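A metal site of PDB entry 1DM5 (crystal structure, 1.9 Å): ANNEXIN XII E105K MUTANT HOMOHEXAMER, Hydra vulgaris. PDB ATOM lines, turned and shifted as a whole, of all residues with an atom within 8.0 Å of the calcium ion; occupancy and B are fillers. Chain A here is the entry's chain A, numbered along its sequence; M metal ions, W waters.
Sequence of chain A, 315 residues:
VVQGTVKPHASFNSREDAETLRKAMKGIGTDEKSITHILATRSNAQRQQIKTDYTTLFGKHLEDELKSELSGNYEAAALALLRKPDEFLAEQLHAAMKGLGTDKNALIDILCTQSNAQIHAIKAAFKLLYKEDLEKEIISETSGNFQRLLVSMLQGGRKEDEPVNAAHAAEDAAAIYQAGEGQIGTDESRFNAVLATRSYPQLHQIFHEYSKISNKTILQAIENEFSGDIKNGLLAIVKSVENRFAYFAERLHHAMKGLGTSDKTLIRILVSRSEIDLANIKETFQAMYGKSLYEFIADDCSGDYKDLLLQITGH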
ATOM      1  N   ILE A 176      36.199   0.818 -12.348  1.00  0.00           N
ATOM      2  CA  ILE A 176      34.981   1.371 -11.751  1.00  0.00           C
ATOM      3  C   ILE A 176      34.491   2.554 -12.559  1.00  0.00           C
ATOM      4  O   ILE A 176      33.293   2.708 -12.826  1.00  0.00           O
ATOM      5  CB  ILE A 176      35.283   1.793 -10.307  1.00  0.00           C
ATOM      6  CG1 ILE A 176      35.626   0.603  -9.387  1.00  0.00           C
ATOM      7  CG2 ILE A 176      34.162   2.610  -9.697  1.00  0.00           C
ATOM      8  CD1 ILE A 176      35.940   1.075  -7.975  1.00  0.00           C
ATOM      9  N   TYR A 177      35.399   3.426 -12.994  1.00  0.00           N
ATOM     10  CA  TYR A 177      35.014   4.544 -13.859  1.00  0.00           C
ATOM     11  C   TYR A 177      34.346   4.036 -15.132  1.00  0.00           C
ATOM     12  O   TYR A 177      33.227   4.444 -15.452  1.00  0.00           O
ATOM     13  CB  TYR A 177      36.252   5.369 -14.224  1.00  0.00           C
ATOM     14  CG  TYR A 177      35.960   6.590 -15.071  1.00  0.00           C
ATOM     15  CD1 TYR A 177      35.615   7.787 -14.458  1.00  0.00           C
ATOM     16  CD2 TYR A 177      36.038   6.549 -16.444  1.00  0.00           C
ATOM     17  CE1 TYR A 177      35.338   8.926 -15.192  1.00  0.00           C
ATOM     18  CE2 TYR A 177      35.776   7.684 -17.197  1.00  0.00           C
ATOM     19  CZ  TYR A 177      35.431   8.869 -16.566  1.00  0.00           C
ATOM     20  OH  TYR A 177      35.171   9.994 -17.310  1.00  0.00           O
ATOM     21  N   GLN A 178      35.030   3.127 -15.817  1.00  0.00           N
ATOM     22  CA  GLN A 178      34.498   2.521 -17.035  1.00  0.00           C
ATOM     23  C   GLN A 178      33.172   1.805 -16.779  1.00  0.00           C
ATOM     24  O   GLN A 178      32.390   1.594 -17.706  1.00  0.00           O
ATOM     25  CB  GLN A 178      35.499   1.537 -17.636  1.00  0.00           C
ATOM     26  CG  GLN A 178      36.707   2.212 -18.274  1.00  0.00           C
ATOM     27  CD  GLN A 178      36.330   3.111 -19.446  1.00  0.00           C
ATOM     28  OE1 GLN A 178      36.614   4.312 -19.418  1.00  0.00           O
ATOM     29  NE2 GLN A 178      35.687   2.530 -20.451  1.00  0.00           N
ATOM     30  N   ALA A 179      32.979   1.399 -15.530  1.00  0.00           N
ATOM     31  CA  ALA A 179      31.830   0.647 -15.080  1.00  0.00           C
ATOM     32  C   ALA A 179      30.588   1.521 -14.999  1.00  0.00           C
ATOM     33  O   ALA A 179      29.473   1.029 -15.097  1.00  0.00           O
ATOM     34  CB  ALA A 179      32.093   0.028 -13.707  1.00  0.00           C
ATOM     35  N   GLY A 180      30.821   2.806 -14.721  1.00  0.00           N
ATOM     36  CA  GLY A 180      29.739   3.740 -14.506  1.00  0.00           C
ATOM     37  C   GLY A 180      29.872   4.957 -15.406  1.00  0.00           C
ATOM     38  O   GLY A 180      29.329   4.969 -16.501  1.00  0.00           O
ATOM     39  N   GLU A 181      30.615   5.969 -14.965  1.00  0.00           N
ATOM     40  CA  GLU A 181      30.780   7.184 -15.748  1.00  0.00           C
ATOM     41  C   GLU A 181      31.219   6.909 -17.188  1.00  0.00           C
ATOM     42  O   GLU A 181      30.764   7.547 -18.136  1.00  0.00           O
ATOM     43  CB  GLU A 181      31.798   8.104 -15.088  1.00  0.00           C
ATOM     44  CG  GLU A 181      31.366   8.744 -13.775  1.00  0.00           C
ATOM     45  CD  GLU A 181      32.395   9.766 -13.344  1.00  0.00           C
ATOM     46  OE1 GLU A 181      33.281   9.430 -12.525  1.00  0.00           O
ATOM     47  OE2 GLU A 181      32.364  10.874 -13.925  1.00  0.00           O
ATOM     48  N   GLY A 182      32.131   5.957 -17.368  1.00  0.00           N
ATOM     49  CA  GLY A 182      32.696   5.709 -18.674  1.00  0.00           C
ATOM     50  C   GLY A 182      31.734   5.275 -19.753  1.00  0.00           C
ATOM     51  O   GLY A 182      32.099   5.255 -20.930  1.00  0.00           O
ATOM     52  N   GLN A 183      30.510   4.920 -19.386  1.00  0.00           N
ATOM     53  CA  GLN A 183      29.576   4.323 -20.343  1.00  0.00           C
ATOM     54  C   GLN A 183      28.155   4.771 -20.076  1.00  0.00           C
ATOM     55  O   GLN A 183      27.860   5.380 -19.045  1.00  0.00           O
ATOM     56  CB  GLN A 183      29.684   2.798 -20.283  1.00  0.00           C
ATOM     57  CG  GLN A 183      29.249   2.216 -18.931  1.00  0.00           C
ATOM     58  CD  GLN A 183      29.009   0.729 -19.006  1.00  0.00           C
ATOM     59  OE1 GLN A 183      27.885   0.279 -19.242  1.00  0.00           O
ATOM     60  NE2 GLN A 183      30.056  -0.071 -18.797  1.00  0.00           N
ATOM     61  N   ILE A 184      27.251   4.478 -21.013  1.00  0.00           N
ATOM     62  CA  ILE A 184      25.863   4.891 -20.920  1.00  0.00           C
ATOM     63  C   ILE A 184      25.108   4.077 -19.863  1.00  0.00           C
ATOM     64  O   ILE A 184      24.485   4.611 -18.940  1.00  0.00           O
ATOM     65  CB  ILE A 184      25.153   4.706 -22.273  1.00  0.00           C
ATOM     66  CG1 ILE A 184      25.679   5.609 -23.390  1.00  0.00           C
ATOM     67  CG2 ILE A 184      23.645   4.852 -22.126  1.00  0.00           C
ATOM     68  CD1 ILE A 184      24.871   6.867 -23.589  1.00  0.00           C
ATOM     69  N   GLY A 185      25.205   2.762 -20.028  1.00  0.00           N
ATOM     70  CA  GLY A 185      24.655   1.788 -19.119  1.00  0.00           C
ATOM     71  C   GLY A 185      25.605   1.554 -17.960  1.00  0.00           C
ATOM     72  O   GLY A 185      26.565   2.312 -17.751  1.00  0.00           O
ATOM     73  N   THR A 186      25.375   0.488 -17.193  1.00  0.00           N
ATOM     74  CA  THR A 186      26.235   0.266 -16.024  1.00  0.00           C
ATOM     75  C   THR A 186      26.769  -1.150 -15.980  1.00  0.00           C
ATOM     76  O   THR A 186      26.191  -2.023 -16.622  1.00  0.00           O
ATOM     77  CB  THR A 186      25.403   0.580 -14.766  1.00  0.00           C
ATOM     78  OG1 THR A 186      25.099   1.983 -14.770  1.00  0.00           O
ATOM     79  CG2 THR A 186      26.181   0.288 -13.496  1.00  0.00           C
ATOM     80  N   ASP A 187      27.889  -1.361 -15.314  1.00  0.00           N
ATOM     81  CA  ASP A 187      28.391  -2.676 -14.922  1.00  0.00           C
ATOM     82  C   ASP A 187      28.430  -2.698 -13.388  1.00  0.00           C
ATOM     83  O   ASP A 187      29.495  -2.612 -12.797  1.00  0.00           O
ATOM     84  CB  ASP A 187      29.780  -2.988 -15.468  1.00  0.00           C
ATOM     85  CG  ASP A 187      30.218  -4.402 -15.141  1.00  0.00           C
ATOM     86  OD1 ASP A 187      31.335  -4.775 -15.552  1.00  0.00           O
ATOM     87  OD2 ASP A 187      29.455  -5.125 -14.469  1.00  0.00           O
ATOM     88  N   GLU A 188      27.253  -2.724 -12.791  1.00  0.00           N
ATOM     89  CA  GLU A 188      27.065  -2.672 -11.360  1.00  0.00           C
ATOM     90  C   GLU A 188      27.933  -3.710 -10.650  1.00  0.00           C
ATOM     91  O   GLU A 188      28.378  -3.537  -9.509  1.00  0.00           O
ATOM     92  CB  GLU A 188      25.614  -2.906 -10.945  1.00  0.00           C
ATOM     93  CG  GLU A 188      24.596  -2.015 -11.627  1.00  0.00           C
ATOM     94  CD  GLU A 188      24.200  -2.474 -13.018  1.00  0.00           C
ATOM     95  OE1 GLU A 188      23.220  -3.240 -13.108  1.00  0.00           O
ATOM     96  OE2 GLU A 188      24.832  -2.055 -14.020  1.00  0.00           O
ATOM     97  N   PHE A 191      31.286  -2.521  -9.397  1.00  0.00           N
ATOM     98  CA  PHE A 191      31.209  -1.747  -8.157  1.00  0.00           C
ATOM     99  C   PHE A 191      31.151  -2.696  -6.961  1.00  0.00           C
ATOM    100  O   PHE A 191      31.805  -2.504  -5.942  1.00  0.00           O
ATOM    101  CB  PHE A 191      29.992  -0.835  -8.149  1.00  0.00           C
ATOM    102  CG  PHE A 191      30.189   0.456  -8.947  1.00  0.00           C
ATOM    103  CD1 PHE A 191      30.443   1.643  -8.282  1.00  0.00           C
ATOM    104  CD2 PHE A 191      30.128   0.454 -10.324  1.00  0.00           C
ATOM    105  CE1 PHE A 191      30.616   2.821  -8.988  1.00  0.00           C
ATOM    106  CE2 PHE A 191      30.274   1.625 -11.045  1.00  0.00           C
ATOM    107  CZ  PHE A 191      30.515   2.818 -10.371  1.00  0.00           C
ATOM    108  N   ALA A 221      29.936   9.725  -7.966  1.00  0.00           N
ATOM    109  CA  ALA A 221      29.657   8.833  -9.100  1.00  0.00           C
ATOM    110  C   ALA A 221      28.567   7.821  -8.712  1.00  0.00           C
ATOM    111  O   ALA A 221      27.594   7.620  -9.430  1.00  0.00           O
ATOM    112  CB  ALA A 221      30.924   8.120  -9.531  1.00  0.00           C
ATOM    113  N   ASN A 224      25.317   9.178  -8.513  1.00  0.00           N
ATOM    114  CA  ASN A 224      24.885   9.464  -9.858  1.00  0.00           C
ATOM    115  C   ASN A 224      24.453   8.230 -10.636  1.00  0.00           C
ATOM    116  O   ASN A 224      23.520   8.325 -11.427  1.00  0.00           O
ATOM    117  CB  ASN A 224      25.995  10.195 -10.633  1.00  0.00           C
ATOM    118  CG  ASN A 224      25.409  11.224 -11.581  1.00  0.00           C
ATOM    119  OD1 ASN A 224      25.320  12.407 -11.240  1.00  0.00           O
ATOM    120  ND2 ASN A 224      24.984  10.765 -12.761  1.00  0.00           N
ATOM    121  N   GLU A 225      25.166   7.130 -10.417  1.00  0.00           N
ATOM    122  CA  GLU A 225      24.994   5.879 -11.131  1.00  0.00           C
ATOM    123  C   GLU A 225      23.822   5.042 -10.646  1.00  0.00           C
ATOM    124  O   GLU A 225      23.257   4.271 -11.414  1.00  0.00           O
ATOM    125  CB  GLU A 225      26.268   5.028 -11.030  1.00  0.00           C
ATOM    126  CG  GLU A 225      26.466   4.038 -12.163  1.00  0.00           C
ATOM    127  CD  GLU A 225      26.545   4.716 -13.530  1.00  0.00           C
ATOM    128  OE1 GLU A 225      27.196   5.777 -13.646  1.00  0.00           O
ATOM    129  OE2 GLU A 225      25.930   4.180 -14.474  1.00  0.00           O
ATOM    130  N   PHE A 226      23.495   5.117  -9.363  1.00  0.00           N
ATOM    131  CA  PHE A 226      22.566   4.177  -8.758  1.00  0.00           C
ATOM    132  C   PHE A 226      21.469   4.889  -7.987  1.00  0.00           C
ATOM    133  O   PHE A 226      21.588   6.081  -7.688  1.00  0.00           O
ATOM    134  CB  PHE A 226      23.305   3.297  -7.736  1.00  0.00           C
ATOM    135  CG  PHE A 226      24.422   2.483  -8.387  1.00  0.00           C
ATOM    136  CD1 PHE A 226      24.094   1.452  -9.253  1.00  0.00           C
ATOM    137  CD2 PHE A 226      25.748   2.798  -8.153  1.00  0.00           C
ATOM    138  CE1 PHE A 226      25.088   0.757  -9.903  1.00  0.00           C
ATOM    139  CE2 PHE A 226      26.745   2.080  -8.775  1.00  0.00           C
ATOM    140  CZ  PHE A 226      26.413   1.058  -9.640  1.00  0.00           C
HETATM  141 CA    CA M   1      26.799   4.452 -16.557  1.00  0.00          CA
HETATM  142  O   HOH W   1      26.536   6.815 -16.317  1.00  0.00           O
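Merely in contact with the calcium ion: Ile 184 (3.3 Å) and Thr 186 (3.5 Å).
O of Gly 185 lies close to OE1 of Gln 183, 2.8 Å away. The side-chain amide oxygen (OE1) of Gln 183 lies within hydrogen-bond range of the backbone NH (N) of Thr 186 (3.2 Å). The backbone carbonyl oxygen (O) of Gln 178 sits at hydrogen-bond distance from the side-chain amide nitrogen (NE2) of Gln 183, at 3.1 Å.
The calcium ion is bound by the side-chain carboxylate (OE2) of Glu 225 (2.3 Å), water W1 (2.4 Å), the backbone carbonyl oxygen (O) of Gly 185 (2.5 Å), the backbone carbonyl oxygen (O) of Gly 180 (2.6 Å) and the backbone carbonyl oxygen (O) of Gln 183 (2.9 Å). The calcium ion has five donor atoms within binding distance.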
